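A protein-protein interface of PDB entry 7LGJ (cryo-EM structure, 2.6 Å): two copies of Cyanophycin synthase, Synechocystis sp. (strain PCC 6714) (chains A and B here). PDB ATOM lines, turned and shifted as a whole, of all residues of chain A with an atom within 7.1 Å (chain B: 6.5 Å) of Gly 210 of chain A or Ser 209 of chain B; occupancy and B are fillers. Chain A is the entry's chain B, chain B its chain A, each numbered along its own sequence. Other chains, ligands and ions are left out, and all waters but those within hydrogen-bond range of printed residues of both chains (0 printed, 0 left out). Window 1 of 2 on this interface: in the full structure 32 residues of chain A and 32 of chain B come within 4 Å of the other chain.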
ATOM      1  N   LEU A 205      27.549  20.269  -2.288  1.00  0.00           N
ATOM      2  CA  LEU A 205      26.114  20.200  -2.573  1.00  0.00           C
ATOM      3  C   LEU A 205      25.557  21.604  -2.594  1.00  0.00           C
ATOM      4  O   LEU A 205      26.017  22.478  -1.863  1.00  0.00           O
ATOM      5  CB  LEU A 205      25.327  19.372  -1.547  1.00  0.00           C
ATOM      6  CG  LEU A 205      25.599  17.879  -1.450  1.00  0.00           C
ATOM      7  CD1 LEU A 205      24.851  17.330  -0.270  1.00  0.00           C
ATOM      8  CD2 LEU A 205      25.089  17.183  -2.715  1.00  0.00           C
ATOM      9  N   SER A 206      24.536  21.835  -3.395  1.00  0.00           N
ATOM     10  CA  SER A 206      23.931  23.157  -3.437  1.00  0.00           C
ATOM     11  C   SER A 206      22.435  23.090  -3.543  1.00  0.00           C
ATOM     12  O   SER A 206      21.839  22.025  -3.693  1.00  0.00           O
ATOM     13  CB  SER A 206      24.446  23.961  -4.609  1.00  0.00           C
ATOM     14  OG  SER A 206      23.929  23.493  -5.813  1.00  0.00           O
ATOM     15  N   SER A 207      21.832  24.257  -3.539  1.00  0.00           N
ATOM     16  CA  SER A 207      20.405  24.464  -3.690  1.00  0.00           C
ATOM     17  C   SER A 207      19.858  23.971  -5.043  1.00  0.00           C
ATOM     18  O   SER A 207      18.645  23.849  -5.214  1.00  0.00           O
ATOM     19  CB  SER A 207      20.114  25.933  -3.504  1.00  0.00           C
ATOM     20  OG  SER A 207      20.806  26.656  -4.476  1.00  0.00           O
ATOM     21  N   HIS A 208      20.744  23.692  -6.005  1.00  0.00           N
ATOM     22  CA  HIS A 208      20.378  23.167  -7.318  1.00  0.00           C
ATOM     23  C   HIS A 208      20.532  21.648  -7.438  1.00  0.00           C
ATOM     24  O   HIS A 208      20.222  21.075  -8.484  1.00  0.00           O
ATOM     25  CB  HIS A 208      21.244  23.808  -8.404  1.00  0.00           C
ATOM     26  CG  HIS A 208      20.954  25.224  -8.687  1.00  0.00           C
ATOM     27  ND1 HIS A 208      20.398  25.629  -9.866  1.00  0.00           N
ATOM     28  CD2 HIS A 208      21.088  26.331  -7.946  1.00  0.00           C
ATOM     29  CE1 HIS A 208      20.234  26.928  -9.847  1.00  0.00           C
ATOM     30  NE2 HIS A 208      20.638  27.375  -8.697  1.00  0.00           N
ATOM     31  N   SER A 209      20.983  20.982  -6.380  1.00  0.00           N
ATOM     32  CA  SER A 209      21.195  19.545  -6.428  1.00  0.00           C
ATOM     33  C   SER A 209      19.954  18.828  -5.946  1.00  0.00           C
ATOM     34  O   SER A 209      19.516  19.053  -4.811  1.00  0.00           O
ATOM     35  CB  SER A 209      22.378  19.128  -5.564  1.00  0.00           C
ATOM     36  OG  SER A 209      23.585  19.664  -6.040  1.00  0.00           O
ATOM     37  N   GLY A 210      19.363  18.026  -6.828  1.00  0.00           N
ATOM     38  CA  GLY A 210      18.129  17.321  -6.539  1.00  0.00           C
ATOM     39  C   GLY A 210      18.371  16.061  -5.758  1.00  0.00           C
ATOM     40  O   GLY A 210      19.382  15.386  -5.956  1.00  0.00           O
ATOM     41  N   ILE A 211      17.388  15.688  -4.968  1.00  0.00           N
ATOM     42  CA  ILE A 211      17.482  14.486  -4.172  1.00  0.00           C
ATOM     43  C   ILE A 211      17.372  13.194  -4.959  1.00  0.00           C
ATOM     44  O   ILE A 211      18.002  12.213  -4.589  1.00  0.00           O
ATOM     45  CB  ILE A 211      16.507  14.515  -2.978  1.00  0.00           C
ATOM     46  CG1 ILE A 211      16.934  13.406  -2.001  1.00  0.00           C
ATOM     47  CG2 ILE A 211      15.052  14.394  -3.394  1.00  0.00           C
ATOM     48  CD1 ILE A 211      16.336  13.475  -0.663  1.00  0.00           C
ATOM     49  N   LEU A 212      16.578  13.153  -6.021  1.00  0.00           N
ATOM     50  CA  LEU A 212      16.440  11.892  -6.730  1.00  0.00           C
ATOM     51  C   LEU A 212      17.764  11.516  -7.389  1.00  0.00           C
ATOM     52  O   LEU A 212      18.145  10.345  -7.389  1.00  0.00           O
ATOM     53  CB  LEU A 212      15.331  11.975  -7.801  1.00  0.00           C
ATOM     54  CG  LEU A 212      13.844  12.165  -7.316  1.00  0.00           C
ATOM     55  CD1 LEU A 212      12.934  12.333  -8.522  1.00  0.00           C
ATOM     56  CD2 LEU A 212      13.382  11.011  -6.501  1.00  0.00           C
ATOM     57  N   GLY A 213      18.466  12.516  -7.924  1.00  0.00           N
ATOM     58  CA  GLY A 213      19.756  12.342  -8.579  1.00  0.00           C
ATOM     59  C   GLY A 213      20.820  11.889  -7.601  1.00  0.00           C
ATOM     60  O   GLY A 213      21.565  10.944  -7.870  1.00  0.00           O
ATOM     61  N   VAL A 214      20.889  12.549  -6.444  1.00  0.00           N
ATOM     62  CA  VAL A 214      21.889  12.206  -5.458  1.00  0.00           C
ATOM     63  C   VAL A 214      21.660  10.811  -4.916  1.00  0.00           C
ATOM     64  O   VAL A 214      22.621  10.073  -4.732  1.00  0.00           O
ATOM     65  CB  VAL A 214      21.938  13.239  -4.313  1.00  0.00           C
ATOM     66  CG1 VAL A 214      22.866  12.757  -3.207  1.00  0.00           C
ATOM     67  CG2 VAL A 214      22.431  14.578  -4.847  1.00  0.00           C
ATOM     68  N   GLU A 215      20.411  10.430  -4.623  1.00  0.00           N
ATOM     69  CA  GLU A 215      20.187   9.077  -4.143  1.00  0.00           C
ATOM     70  C   GLU A 215      20.493   8.020  -5.196  1.00  0.00           C
ATOM     71  O   GLU A 215      21.082   6.998  -4.871  1.00  0.00           O
ATOM     72  CB  GLU A 215      18.775   8.878  -3.648  1.00  0.00           C
ATOM     73  CG  GLU A 215      18.440   9.569  -2.356  1.00  0.00           C
ATOM     74  CD  GLU A 215      17.026   9.267  -1.895  1.00  0.00           C
ATOM     75  OE1 GLU A 215      16.248   8.732  -2.674  1.00  0.00           O
ATOM     76  OE2 GLU A 215      16.726   9.552  -0.760  1.00  0.00           O
ATOM     77  N   GLY A 424      20.857  12.564 -13.573  1.00  0.00           N
ATOM     78  CA  GLY A 424      20.404  13.738 -12.861  1.00  0.00           C
ATOM     79  C   GLY A 424      21.128  14.552 -11.808  1.00  0.00           C
ATOM     80  O   GLY A 424      20.493  15.075 -10.895  1.00  0.00           O
ATOM     81  N   LEU A 425      22.447  14.678 -11.983  1.00  0.00           N
ATOM     82  CA  LEU A 425      23.294  15.397 -10.999  1.00  0.00           C
ATOM     83  C   LEU A 425      23.902  16.636 -11.647  1.00  0.00           C
ATOM     84  O   LEU A 425      24.390  16.512 -12.789  1.00  0.00           O
ATOM     85  CB  LEU A 425      24.455  14.467 -10.653  1.00  0.00           C
ATOM     86  CG  LEU A 425      24.166  13.387  -9.622  1.00  0.00           C
ATOM     87  CD1 LEU A 425      25.394  12.515  -9.450  1.00  0.00           C
ATOM     88  CD2 LEU A 425      23.771  14.028  -8.306  1.00  0.00           C
ATOM     89  N   ASP A 426      23.893  17.773 -10.950  1.00  0.00           N
ATOM     90  CA  ASP A 426      24.616  18.923 -11.484  1.00  0.00           C
ATOM     91  C   ASP A 426      26.120  18.882 -11.302  1.00  0.00           C
ATOM     92  O   ASP A 426      26.849  18.845 -12.288  1.00  0.00           O
ATOM     93  CB  ASP A 426      24.025  20.205 -10.907  1.00  0.00           C
ATOM     94  CG  ASP A 426      24.035  20.245  -9.406  1.00  0.00           C
ATOM     95  OD1 ASP A 426      24.184  19.176  -8.786  1.00  0.00           O
ATOM     96  OD2 ASP A 426      23.927  21.310  -8.865  1.00  0.00           O
ATOM     97  N   THR B 204       5.939  11.317  -3.678  1.00  0.00           N
ATOM     98  CA  THR B 204       5.787  12.735  -3.404  1.00  0.00           C
ATOM     99  C   THR B 204       7.068  13.576  -3.510  1.00  0.00           C
ATOM    100  O   THR B 204       7.085  14.740  -3.118  1.00  0.00           O
ATOM    101  CB  THR B 204       5.056  12.860  -2.067  1.00  0.00           C
ATOM    102  OG1 THR B 204       5.770  12.075  -1.078  1.00  0.00           O
ATOM    103  CG2 THR B 204       3.648  12.328  -2.256  1.00  0.00           C
ATOM    104  N   LEU B 205       8.147  12.974  -4.009  1.00  0.00           N
ATOM    105  CA  LEU B 205       9.402  13.665  -4.316  1.00  0.00           C
ATOM    106  C   LEU B 205       9.494  13.858  -5.812  1.00  0.00           C
ATOM    107  O   LEU B 205       9.020  13.031  -6.587  1.00  0.00           O
ATOM    108  CB  LEU B 205      10.650  12.909  -3.838  1.00  0.00           C
ATOM    109  CG  LEU B 205      10.865  12.726  -2.344  1.00  0.00           C
ATOM    110  CD1 LEU B 205      12.037  11.812  -2.136  1.00  0.00           C
ATOM    111  CD2 LEU B 205      11.184  14.079  -1.704  1.00  0.00           C
ATOM    112  N   SER B 206      10.137  14.924  -6.243  1.00  0.00           N
ATOM    113  CA  SER B 206      10.293  15.150  -7.672  1.00  0.00           C
ATOM    114  C   SER B 206      11.651  15.689  -8.014  1.00  0.00           C
ATOM    115  O   SER B 206      12.468  15.999  -7.148  1.00  0.00           O
ATOM    116  CB  SER B 206       9.260  16.126  -8.189  1.00  0.00           C
ATOM    117  OG  SER B 206       9.536  17.426  -7.775  1.00  0.00           O
ATOM    118  N   SER B 207      11.862  15.870  -9.298  1.00  0.00           N
ATOM    119  CA  SER B 207      13.066  16.433  -9.879  1.00  0.00           C
ATOM    120  C   SER B 207      13.335  17.882  -9.436  1.00  0.00           C
ATOM    121  O   SER B 207      14.433  18.400  -9.641  1.00  0.00           O
ATOM    122  CB  SER B 207      12.953  16.349 -11.382  1.00  0.00           C
ATOM    123  OG  SER B 207      11.838  17.081 -11.792  1.00  0.00           O
ATOM    124  N   HIS B 208      12.339  18.541  -8.834  1.00  0.00           N
ATOM    125  CA  HIS B 208      12.463  19.900  -8.313  1.00  0.00           C
ATOM    126  C   HIS B 208      12.735  19.959  -6.807  1.00  0.00           C
ATOM    127  O   HIS B 208      12.895  21.046  -6.250  1.00  0.00           O
ATOM    128  CB  HIS B 208      11.181  20.690  -8.585  1.00  0.00           C
ATOM    129  CG  HIS B 208      10.953  21.055  -9.994  1.00  0.00           C
ATOM    130  ND1 HIS B 208      11.016  22.349 -10.427  1.00  0.00           N
ATOM    131  CD2 HIS B 208      10.712  20.315 -11.083  1.00  0.00           C
ATOM    132  CE1 HIS B 208      10.791  22.386 -11.716  1.00  0.00           C
ATOM    133  NE2 HIS B 208      10.609  21.173 -12.137  1.00  0.00           N
ATOM    134  N   SER B 209      12.810  18.811  -6.143  1.00  0.00           N
ATOM    135  CA  SER B 209      13.024  18.786  -4.704  1.00  0.00           C
ATOM    136  C   SER B 209      14.503  18.683  -4.409  1.00  0.00           C
ATOM    137  O   SER B 209      15.152  17.726  -4.851  1.00  0.00           O
ATOM    138  CB  SER B 209      12.303  17.611  -4.056  1.00  0.00           C
ATOM    139  OG  SER B 209      10.909  17.717  -4.189  1.00  0.00           O
ATOM    140  N   GLY B 210      15.035  19.693  -3.725  1.00  0.00           N
ATOM    141  CA  GLY B 210      16.451  19.772  -3.421  1.00  0.00           C
ATOM    142  C   GLY B 210      16.814  18.946  -2.221  1.00  0.00           C
ATOM    143  O   GLY B 210      16.032  18.836  -1.276  1.00  0.00           O
ATOM    144  N   ILE B 211      18.043  18.476  -2.211  1.00  0.00           N
ATOM    145  CA  ILE B 211      18.530  17.679  -1.109  1.00  0.00           C
ATOM    146  C   ILE B 211      18.790  18.454   0.168  1.00  0.00           C
ATOM    147  O   ILE B 211      18.604  17.910   1.247  1.00  0.00           O
ATOM    148  CB  ILE B 211      19.745  16.822  -1.518  1.00  0.00           C
ATOM    149  CG1 ILE B 211      19.950  15.755  -0.429  1.00  0.00           C
ATOM    150  CG2 ILE B 211      20.996  17.644  -1.768  1.00  0.00           C
ATOM    151  CD1 ILE B 211      20.849  14.651  -0.784  1.00  0.00           C
ATOM    152  N   VAL B 214      15.350  18.843   1.901  1.00  0.00           N
ATOM    153  CA  VAL B 214      14.809  17.604   2.415  1.00  0.00           C
ATOM    154  C   VAL B 214      15.578  17.144   3.636  1.00  0.00           C
ATOM    155  O   VAL B 214      14.966  16.681   4.592  1.00  0.00           O
ATOM    156  CB  VAL B 214      14.779  16.503   1.336  1.00  0.00           C
ATOM    157  CG1 VAL B 214      14.378  15.170   1.954  1.00  0.00           C
ATOM    158  CG2 VAL B 214      13.787  16.878   0.243  1.00  0.00           C
ATOM    159  N   GLY B 424      13.395  25.670   2.532  1.00  0.00           N
ATOM    160  CA  GLY B 424      13.663  25.129   1.218  1.00  0.00           C
ATOM    161  C   GLY B 424      13.055  23.915   0.545  1.00  0.00           C
ATOM    162  O   GLY B 424      13.736  23.231  -0.216  1.00  0.00           O
ATOM    163  N   LEU B 425      11.762  23.699   0.808  1.00  0.00           N
ATOM    164  CA  LEU B 425      11.051  22.515   0.265  1.00  0.00           C
ATOM    165  C   LEU B 425       9.951  22.965  -0.690  1.00  0.00           C
ATOM    166  O   LEU B 425       9.225  23.914  -0.331  1.00  0.00           O
ATOM    167  CB  LEU B 425      10.357  21.838   1.447  1.00  0.00           C
ATOM    168  CG  LEU B 425      11.224  20.930   2.303  1.00  0.00           C
ATOM    169  CD1 LEU B 425      10.403  20.400   3.464  1.00  0.00           C
ATOM    170  CD2 LEU B 425      11.762  19.791   1.459  1.00  0.00           C
ATOM    171  N   ASP B 426       9.820  22.308  -1.844  1.00  0.00           N
ATOM    172  CA  ASP B 426       8.673  22.616  -2.693  1.00  0.00           C
ATOM    173  C   ASP B 426       7.359  22.003  -2.252  1.00  0.00           C
ATOM    174  O   ASP B 426       6.429  22.731  -1.923  1.00  0.00           O
ATOM    175  CB  ASP B 426       8.999  22.246  -4.137  1.00  0.00           C
ATOM    176  CG  ASP B 426       9.393  20.808  -4.310  1.00  0.00           C
ATOM    177  OD1 ASP B 426       9.743  20.164  -3.304  1.00  0.00           O
ATOM    178  OD2 ASP B 426       9.332  20.330  -5.408  1.00  0.00           O
ATOM    179  N   ILE B 427       7.311  20.692  -2.117  1.00  0.00           N
ATOM    180  CA  ILE B 427       6.076  20.096  -1.645  1.00  0.00           C
ATOM    181  C   ILE B 427       6.264  19.763  -0.181  1.00  0.00           C
ATOM    182  O   ILE B 427       7.095  18.914   0.179  1.00  0.00           O
ATOM    183  CB  ILE B 427       5.662  18.844  -2.433  1.00  0.00           C
ATOM    184  CG1 ILE B 427       5.509  19.208  -3.901  1.00  0.00           C
ATOM    185  CG2 ILE B 427       4.315  18.346  -1.882  1.00  0.00           C
ATOM    186  CD1 ILE B 427       5.327  18.053  -4.838  1.00  0.00           C
ATOM    187  N   MET B 478       3.719  22.891 -11.749  1.00  0.00           N
ATOM    188  CA  MET B 478       5.058  23.421 -11.541  1.00  0.00           C
ATOM    189  C   MET B 478       6.031  22.653 -12.421  1.00  0.00           C
ATOM    190  O   MET B 478       7.010  23.214 -12.907  1.00  0.00           O
ATOM    191  CB  MET B 478       5.516  23.384 -10.075  1.00  0.00           C
ATOM    192  CG  MET B 478       5.937  22.055  -9.560  1.00  0.00           C
ATOM    193  SD  MET B 478       6.457  22.047  -7.885  1.00  0.00           S
ATOM    194  CE  MET B 478       6.726  20.305  -7.775  1.00  0.00           C
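Among the printed residues, pairs that only touch across the chains: Ser 209 of chain A with Gly 210 of chain B (3.4 Å), Gly 210 of chain A with Ser 209 of chain B (3.4 Å), Ile 211 of chain A with Ile 211 of chain B (3.98 Å), Ile 211 of chain A with Val 214 of chain B (3.7 Å), Leu 212 of chain A with Ser 206 of chain B (3.6 Å), Leu 212 of chain A with Ser 207 of chain B (3.8 Å) and Val 214 of chain A with Ile 211 of chain B (3.7 Å).
Of the 14 printed residues of chain B, 6 touch a printed residue of chain A.
Hydrophobic or aromatic side chains of chain B that line the printed part of chain A: Ile 211 and Val 214.
Hydrophobic or aromatic side chains of chain A within 4 Å of the printed part of chain B: Ile 211, Leu 212 and Val 214.
Along chain A the printed residues that touch a printed residue of chain B span positions 209 to 214.
Of the printed residues of chain B, Ser 209 of chain A touches Gly 210 (3.4 Å) and Ile 211 (3.0 Å).
Gly 210 of chain A touches just one residue of chain B: Ser 209.
Thr 204 of chain B touches none of the printed residues of chain A.
Of the printed residues of chain A, Ser 207 of chain B touches Leu 212 (3.8 Å).
Of chain A, only Gly 210 and Ile 211 come within 4 Å of Ser 209 of chain B.
Printed residues of chain A within 4 Å of Gly 210 of chain B: Ser 209 (3.4 Å).
Asp 426 of chain B touches none of the printed residues of chain A.
The nearest printed residue of chain B that does not touch Gly 210 of chain A is Ile 211 of chain B (4.3 Å).
The nearest printed residue of chain A that does not touch Gly 210 of chain B is Ile 211 of chain A (4.3 Å).
The side-chain hydroxyl of Ser 206 of chain B lies close to the backbone NH of His 208 of chain B.
OG of Ser 209 of chain B lies within hydrogen-bond range of OD1 of Asp 426 of chain B (2.9 Å).
OG of Ser 209 of chain A is in hydrogen-bond range of OD1 of Asp 426 of chain A.
The backbone carbonyl oxygen (O) of Ser 209 of chain B lies within hydrogen-bond range of the backbone NH (N) of Ile 211 of chain A (3.0 Å).
The backbone NH of Ile 211 of chain B sits at hydrogen-bond distance from the backbone carbonyl oxygen of Ser 209 of chain A, 3.0 Å away.
Ser 209 of chain A touches Gly 210 of chain B, and with the chains exchanged Gly 210 of chain A touches Ser 209 of chain B.
Ser 209 of chain A touches Ile 211 of chain B, and with the chains exchanged Ile 211 of chain A touches Ser 209 of chain B.
Ile 211 of chain B touches its own counterpart, Ile 211 of chain A.
Ile 211 of chain A touches Val 214 of chain B, and with the chains exchanged Val 214 of chain A touches Ile 211 of chain B.
11 positions are printed for both chains.
Of the 9 pairs that touch across the chains among the printed residues, 7 have their exchanged pair printed and touching as well.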
